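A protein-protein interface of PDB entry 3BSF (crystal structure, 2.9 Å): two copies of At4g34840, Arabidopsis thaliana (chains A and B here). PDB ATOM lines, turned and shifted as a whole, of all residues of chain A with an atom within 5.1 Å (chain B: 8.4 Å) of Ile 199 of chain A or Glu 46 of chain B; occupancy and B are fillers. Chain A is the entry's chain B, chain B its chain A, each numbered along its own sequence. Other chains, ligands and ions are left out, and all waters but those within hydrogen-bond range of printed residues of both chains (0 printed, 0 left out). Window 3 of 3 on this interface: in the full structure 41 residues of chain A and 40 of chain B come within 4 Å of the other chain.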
ATOM      1  N   TYR A 195      -5.469 -30.353  19.217  1.00  0.00           N
ATOM      2  CA  TYR A 195      -4.327 -29.516  18.942  1.00  0.00           C
ATOM      3  C   TYR A 195      -3.478 -29.313  20.180  1.00  0.00           C
ATOM      4  O   TYR A 195      -2.269 -29.525  20.141  1.00  0.00           O
ATOM      5  CB  TYR A 195      -4.776 -28.157  18.434  1.00  0.00           C
ATOM      6  CG  TYR A 195      -3.643 -27.163  18.291  1.00  0.00           C
ATOM      7  CD1 TYR A 195      -2.618 -27.379  17.371  1.00  0.00           C
ATOM      8  CD2 TYR A 195      -3.629 -25.984  19.034  1.00  0.00           C
ATOM      9  CE1 TYR A 195      -1.605 -26.433  17.181  1.00  0.00           C
ATOM     10  CE2 TYR A 195      -2.628 -25.028  18.857  1.00  0.00           C
ATOM     11  CZ  TYR A 195      -1.618 -25.248  17.928  1.00  0.00           C
ATOM     12  OH  TYR A 195      -0.645 -24.275  17.716  1.00  0.00           O
ATOM     13  N   VAL A 196      -4.104 -28.881  21.273  1.00  0.00           N
ATOM     14  CA  VAL A 196      -3.360 -28.636  22.504  1.00  0.00           C
ATOM     15  C   VAL A 196      -2.671 -29.910  23.013  1.00  0.00           C
ATOM     16  O   VAL A 196      -1.443 -29.923  23.197  1.00  0.00           O
ATOM     17  CB  VAL A 196      -4.275 -28.030  23.636  1.00  0.00           C
ATOM     18  CG1 VAL A 196      -3.464 -27.787  24.905  1.00  0.00           C
ATOM     19  CG2 VAL A 196      -4.881 -26.706  23.175  1.00  0.00           C
ATOM     20  N   ALA A 197      -3.442 -30.980  23.215  1.00  0.00           N
ATOM     21  CA  ALA A 197      -2.882 -32.236  23.719  1.00  0.00           C
ATOM     22  C   ALA A 197      -1.723 -32.745  22.855  1.00  0.00           C
ATOM     23  O   ALA A 197      -0.806 -33.426  23.333  1.00  0.00           O
ATOM     24  CB  ALA A 197      -3.969 -33.286  23.809  1.00  0.00           C
ATOM     25  N   ASP A 198      -1.768 -32.390  21.579  1.00  0.00           N
ATOM     26  CA  ASP A 198      -0.754 -32.792  20.621  1.00  0.00           C
ATOM     27  C   ASP A 198       0.568 -32.069  20.850  1.00  0.00           C
ATOM     28  O   ASP A 198       1.622 -32.606  20.533  1.00  0.00           O
ATOM     29  CB  ASP A 198      -1.260 -32.511  19.204  1.00  0.00           C
ATOM     30  CG  ASP A 198      -0.350 -33.065  18.142  1.00  0.00           C
ATOM     31  OD1 ASP A 198      -0.312 -34.305  18.001  1.00  0.00           O
ATOM     32  OD2 ASP A 198       0.332 -32.271  17.454  1.00  0.00           O
ATOM     33  N   ILE A 199       0.521 -30.852  21.391  1.00  0.00           N
ATOM     34  CA  ILE A 199       1.758 -30.106  21.622  1.00  0.00           C
ATOM     35  C   ILE A 199       2.472 -30.715  22.817  1.00  0.00           C
ATOM     36  O   ILE A 199       3.692 -30.822  22.826  1.00  0.00           O
ATOM     37  CB  ILE A 199       1.505 -28.572  21.851  1.00  0.00           C
ATOM     38  CG1 ILE A 199       1.331 -28.265  23.329  1.00  0.00           C
ATOM     39  CG2 ILE A 199       0.268 -28.114  21.103  1.00  0.00           C
ATOM     40  CD1 ILE A 199       2.558 -27.633  23.970  1.00  0.00           C
ATOM     41  N   PHE A 200       1.702 -31.124  23.822  1.00  0.00           N
ATOM     42  CA  PHE A 200       2.268 -31.755  25.007  1.00  0.00           C
ATOM     43  C   PHE A 200       2.340 -33.243  24.749  1.00  0.00           C
ATOM     44  O   PHE A 200       2.555 -34.033  25.665  1.00  0.00           O
ATOM     45  CB  PHE A 200       1.403 -31.492  26.237  1.00  0.00           C
ATOM     46  CG  PHE A 200       1.388 -30.058  26.655  1.00  0.00           C
ATOM     47  CD1 PHE A 200       0.390 -29.202  26.212  1.00  0.00           C
ATOM     48  CD2 PHE A 200       2.410 -29.540  27.453  1.00  0.00           C
ATOM     49  CE1 PHE A 200       0.409 -27.838  26.558  1.00  0.00           C
ATOM     50  CE2 PHE A 200       2.442 -28.184  27.802  1.00  0.00           C
ATOM     51  CZ  PHE A 200       1.435 -27.332  27.351  1.00  0.00           C
ATOM     52  N   LYS A 201       2.143 -33.617  23.490  1.00  0.00           N
ATOM     53  CA  LYS A 201       2.188 -35.014  23.084  1.00  0.00           C
ATOM     54  C   LYS A 201       1.548 -36.009  24.062  1.00  0.00           C
ATOM     55  O   LYS A 201       2.136 -37.037  24.376  1.00  0.00           O
ATOM     56  CB  LYS A 201       3.635 -35.426  22.805  1.00  0.00           C
ATOM     57  CG  LYS A 201       4.026 -35.362  21.326  1.00  0.00           C
ATOM     58  CD  LYS A 201       4.136 -33.931  20.778  1.00  0.00           C
ATOM     59  CE  LYS A 201       4.562 -33.922  19.304  1.00  0.00           C
ATOM     60  NZ  LYS A 201       4.916 -32.553  18.797  1.00  0.00           N
ATOM     61  N   THR B  41      11.996 -18.603  28.180  1.00  0.00           N
ATOM     62  CA  THR B  41      10.682 -18.004  28.255  1.00  0.00           C
ATOM     63  C   THR B  41      10.003 -18.639  29.474  1.00  0.00           C
ATOM     64  O   THR B  41      10.383 -19.728  29.928  1.00  0.00           O
ATOM     65  CB  THR B  41       9.847 -18.247  26.946  1.00  0.00           C
ATOM     66  OG1 THR B  41       9.643 -19.652  26.742  1.00  0.00           O
ATOM     67  CG2 THR B  41      10.564 -17.656  25.733  1.00  0.00           C
ATOM     68  N   PHE B  43       7.364 -19.961  29.564  1.00  0.00           N
ATOM     69  CA  PHE B  43       6.358 -20.870  29.031  1.00  0.00           C
ATOM     70  C   PHE B  43       6.820 -22.323  29.088  1.00  0.00           C
ATOM     71  O   PHE B  43       8.002 -22.607  29.309  1.00  0.00           O
ATOM     72  CB  PHE B  43       6.026 -20.502  27.578  1.00  0.00           C
ATOM     73  CG  PHE B  43       5.711 -19.043  27.374  1.00  0.00           C
ATOM     74  CD1 PHE B  43       4.808 -18.385  28.224  1.00  0.00           C
ATOM     75  CD2 PHE B  43       6.301 -18.331  26.323  1.00  0.00           C
ATOM     76  CE1 PHE B  43       4.492 -17.044  28.036  1.00  0.00           C
ATOM     77  CE2 PHE B  43       5.999 -16.989  26.121  1.00  0.00           C
ATOM     78  CZ  PHE B  43       5.086 -16.336  26.981  1.00  0.00           C
ATOM     79  N   PRO B  44       5.883 -23.269  28.893  1.00  0.00           N
ATOM     80  CA  PRO B  44       6.229 -24.694  28.921  1.00  0.00           C
ATOM     81  C   PRO B  44       7.250 -25.007  27.833  1.00  0.00           C
ATOM     82  O   PRO B  44       7.154 -24.514  26.697  1.00  0.00           O
ATOM     83  CB  PRO B  44       4.892 -25.391  28.659  1.00  0.00           C
ATOM     84  CG  PRO B  44       3.882 -24.424  29.197  1.00  0.00           C
ATOM     85  CD  PRO B  44       4.426 -23.086  28.736  1.00  0.00           C
ATOM     86  N   LYS B  45       8.220 -25.841  28.187  1.00  0.00           N
ATOM     87  CA  LYS B  45       9.276 -26.219  27.264  1.00  0.00           C
ATOM     88  C   LYS B  45       8.724 -26.663  25.899  1.00  0.00           C
ATOM     89  O   LYS B  45       9.386 -26.500  24.875  1.00  0.00           O
ATOM     90  CB  LYS B  45      10.116 -27.328  27.896  1.00  0.00           C
ATOM     91  CG  LYS B  45      11.512 -27.463  27.324  1.00  0.00           C
ATOM     92  CD  LYS B  45      12.493 -28.048  28.366  1.00  0.00           C
ATOM     93  CE  LYS B  45      13.966 -27.861  27.949  1.00  0.00           C
ATOM     94  NZ  LYS B  45      14.950 -28.101  29.056  1.00  0.00           N
ATOM     95  N   GLU B  46       7.500 -27.181  25.864  1.00  0.00           N
ATOM     96  CA  GLU B  46       6.957 -27.669  24.599  1.00  0.00           C
ATOM     97  C   GLU B  46       6.307 -26.711  23.601  1.00  0.00           C
ATOM     98  O   GLU B  46       6.264 -27.014  22.415  1.00  0.00           O
ATOM     99  CB  GLU B  46       6.007 -28.852  24.843  1.00  0.00           C
ATOM    100  CG  GLU B  46       5.348 -28.863  26.185  1.00  0.00           C
ATOM    101  CD  GLU B  46       6.201 -29.535  27.235  1.00  0.00           C
ATOM    102  OE1 GLU B  46       6.480 -30.744  27.067  1.00  0.00           O
ATOM    103  OE2 GLU B  46       6.585 -28.858  28.220  1.00  0.00           O
ATOM    104  N   VAL B  47       5.799 -25.572  24.042  1.00  0.00           N
ATOM    105  CA  VAL B  47       5.189 -24.649  23.087  1.00  0.00           C
ATOM    106  C   VAL B  47       6.268 -24.036  22.223  1.00  0.00           C
ATOM    107  O   VAL B  47       7.438 -24.172  22.538  1.00  0.00           O
ATOM    108  CB  VAL B  47       4.433 -23.517  23.799  1.00  0.00           C
ATOM    109  CG1 VAL B  47       3.366 -24.113  24.711  1.00  0.00           C
ATOM    110  CG2 VAL B  47       5.393 -22.666  24.597  1.00  0.00           C
ATOM    111  N   THR B  48       5.879 -23.362  21.141  1.00  0.00           N
ATOM    112  CA  THR B  48       6.835 -22.721  20.222  1.00  0.00           C
ATOM    113  C   THR B  48       6.814 -21.195  20.338  1.00  0.00           C
ATOM    114  O   THR B  48       7.410 -20.488  19.514  1.00  0.00           O
ATOM    115  CB  THR B  48       6.556 -23.105  18.726  1.00  0.00           C
ATOM    116  OG1 THR B  48       5.238 -22.673  18.334  1.00  0.00           O
ATOM    117  CG2 THR B  48       6.677 -24.605  18.534  1.00  0.00           C
ATOM    118  N   TRP B  49       6.133 -20.701  21.370  1.00  0.00           N
ATOM    119  CA  TRP B  49       6.002 -19.266  21.610  1.00  0.00           C
ATOM    120  C   TRP B  49       7.320 -18.543  21.857  1.00  0.00           C
ATOM    121  O   TRP B  49       8.197 -19.037  22.565  1.00  0.00           O
ATOM    122  CB  TRP B  49       5.061 -19.020  22.786  1.00  0.00           C
ATOM    123  CG  TRP B  49       3.833 -19.857  22.696  1.00  0.00           C
ATOM    124  CD1 TRP B  49       3.315 -20.441  21.560  1.00  0.00           C
ATOM    125  CD2 TRP B  49       2.936 -20.201  23.764  1.00  0.00           C
ATOM    126  NE1 TRP B  49       2.156 -21.125  21.864  1.00  0.00           N
ATOM    127  CE2 TRP B  49       1.902 -20.995  23.206  1.00  0.00           C
ATOM    128  CE3 TRP B  49       2.902 -19.920  25.134  1.00  0.00           C
ATOM    129  CZ2 TRP B  49       0.849 -21.507  23.977  1.00  0.00           C
ATOM    130  CZ3 TRP B  49       1.846 -20.435  25.898  1.00  0.00           C
ATOM    131  CH2 TRP B  49       0.842 -21.218  25.314  1.00  0.00           C
ATOM    132  N   LYS B  68       6.021 -20.078  15.078  1.00  0.00           N
ATOM    133  CA  LYS B  68       5.728 -20.857  13.879  1.00  0.00           C
ATOM    134  C   LYS B  68       5.268 -22.249  14.277  1.00  0.00           C
ATOM    135  O   LYS B  68       5.774 -22.801  15.252  1.00  0.00           O
ATOM    136  CB  LYS B  68       6.983 -20.966  13.003  1.00  0.00           C
ATOM    137  CG  LYS B  68       7.676 -19.634  12.749  1.00  0.00           C
ATOM    138  CD  LYS B  68       7.905 -19.372  11.268  1.00  0.00           C
ATOM    139  CE  LYS B  68       8.507 -17.979  11.030  1.00  0.00           C
ATOM    140  NZ  LYS B  68       8.536 -17.565   9.573  1.00  0.00           N
ATOM    141  N   ASP B  69       4.319 -22.810  13.524  1.00  0.00           N
ATOM    142  CA  ASP B  69       3.778 -24.143  13.806  1.00  0.00           C
ATOM    143  C   ASP B  69       4.896 -25.172  13.769  1.00  0.00           C
ATOM    144  O   ASP B  69       5.726 -25.166  12.858  1.00  0.00           O
ATOM    145  CB  ASP B  69       2.701 -24.533  12.783  1.00  0.00           C
ATOM    146  CG  ASP B  69       1.842 -25.704  13.260  1.00  0.00           C
ATOM    147  OD1 ASP B  69       1.122 -25.521  14.274  1.00  0.00           O
ATOM    148  OD2 ASP B  69       1.883 -26.799  12.642  1.00  0.00           O
ATOM    149  N   SER B  70       4.911 -26.064  14.751  1.00  0.00           N
ATOM    150  CA  SER B  70       5.955 -27.069  14.829  1.00  0.00           C
ATOM    151  C   SER B  70       5.864 -28.135  13.743  1.00  0.00           C
ATOM    152  O   SER B  70       6.822 -28.880  13.534  1.00  0.00           O
ATOM    153  CB  SER B  70       5.932 -27.742  16.198  1.00  0.00           C
ATOM    154  OG  SER B  70       4.732 -28.485  16.368  1.00  0.00           O
ATOM    155  N   SER B  76       1.564 -19.631  13.488  1.00  0.00           N
ATOM    156  CA  SER B  76       0.335 -20.143  14.072  1.00  0.00           C
ATOM    157  C   SER B  76      -0.696 -19.044  14.322  1.00  0.00           C
ATOM    158  O   SER B  76      -0.905 -18.613  15.457  1.00  0.00           O
ATOM    159  CB  SER B  76       0.631 -20.885  15.388  1.00  0.00           C
ATOM    160  OG  SER B  76       0.978 -22.247  15.165  1.00  0.00           O
ATOM    161  N   VAL B  80      -7.370 -19.783  18.238  1.00  0.00           N
ATOM    162  CA  VAL B  80      -6.871 -20.736  19.232  1.00  0.00           C
ATOM    163  C   VAL B  80      -5.466 -20.438  19.776  1.00  0.00           C
ATOM    164  O   VAL B  80      -5.260 -20.436  20.995  1.00  0.00           O
ATOM    165  CB  VAL B  80      -6.914 -22.176  18.703  1.00  0.00           C
ATOM    166  CG1 VAL B  80      -6.081 -23.079  19.590  1.00  0.00           C
ATOM    167  CG2 VAL B  80      -8.370 -22.665  18.687  1.00  0.00           C
ATOM    168  N   LEU B  84      -4.522 -18.987  23.651  1.00  0.00           N
ATOM    169  CA  LEU B  84      -3.567 -19.718  24.477  1.00  0.00           C
ATOM    170  C   LEU B  84      -2.439 -18.783  24.914  1.00  0.00           C
ATOM    171  O   LEU B  84      -2.150 -18.649  26.102  1.00  0.00           O
ATOM    172  CB  LEU B  84      -2.997 -20.918  23.697  1.00  0.00           C
ATOM    173  CG  LEU B  84      -3.982 -22.072  23.443  1.00  0.00           C
ATOM    174  CD1 LEU B  84      -3.305 -23.219  22.678  1.00  0.00           C
ATOM    175  CD2 LEU B  84      -4.525 -22.569  24.778  1.00  0.00           C
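The side-chain carboxylate (OD1) of Asp 69 of chain B sits at hydrogen-bond distance from the side-chain hydroxyl (OG) of Ser 76 of chain B (3.4 Å).
Among the printed residues, pairs that only touch across the chains: Phe 200 of chain A with Glu 46 of chain B, Tyr 195 of chain A with Ser 76 of chain B, Ile 199 of chain A with Glu 46 of chain B, Ile 199 of chain A with Val 47 of chain B, Phe 200 of chain A with Pro 44 of chain B, Tyr 195 of chain A with Val 80 of chain B and Val 196 of chain A with Leu 84 of chain B.
Of chain B, only Glu 46 (3.6 Å) and Val 47 (3.7 Å) come within 4 Å of Ile 199 of chain A. Printed residues of chain A within 4 Å of Glu 46 of chain B: Ile 199 (3.6 Å) and Phe 200 (3.3 Å). Of the printed residues of chain B, Tyr 195 of chain A touches Ser 76 and Val 80. Printed residues of chain A within 4 Å of Val 80 of chain B: Tyr 195. Trp 49 of chain B touches none of the printed residues of chain A. Asp 69 of chain B touches none of the printed residues of chain A. The nearest printed residue of chain A that does not touch Glu 46 of chain B is Lys 201 of chain A (6.3 Å).
Of the 7 printed residues of chain A, 4 touch a printed residue of chain B. Printed residues of chain A that touch a printed residue of chain B: Tyr 195, Val 196, Ile 199 and Phe 200. Hydrophobic or aromatic side chains of chain A within 4 Å of the printed part of chain B: Tyr 195, Val 196, Ile 199 and Phe 200. Printed residues of chain B that touch a printed residue of chain A: Pro 44, Glu 46, Val 47, Ser 76, Val 80 and Leu 84. Hydrophobic or aromatic side chains of chain B within 4 Å of the printed part of chain A: Pro 44, Val 47, Val 80 and Leu 84. Along chain B the printed residues that touch a printed residue of chain A span positions 44 to 84. Among the printed residues, 7 pairs touch across the chains. Among the printed residues, no Asp or Glu carboxylate lies within 4 Å of a Lys or Arg side-chain nitrogen of the other chain.
No position is printed for both chains.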
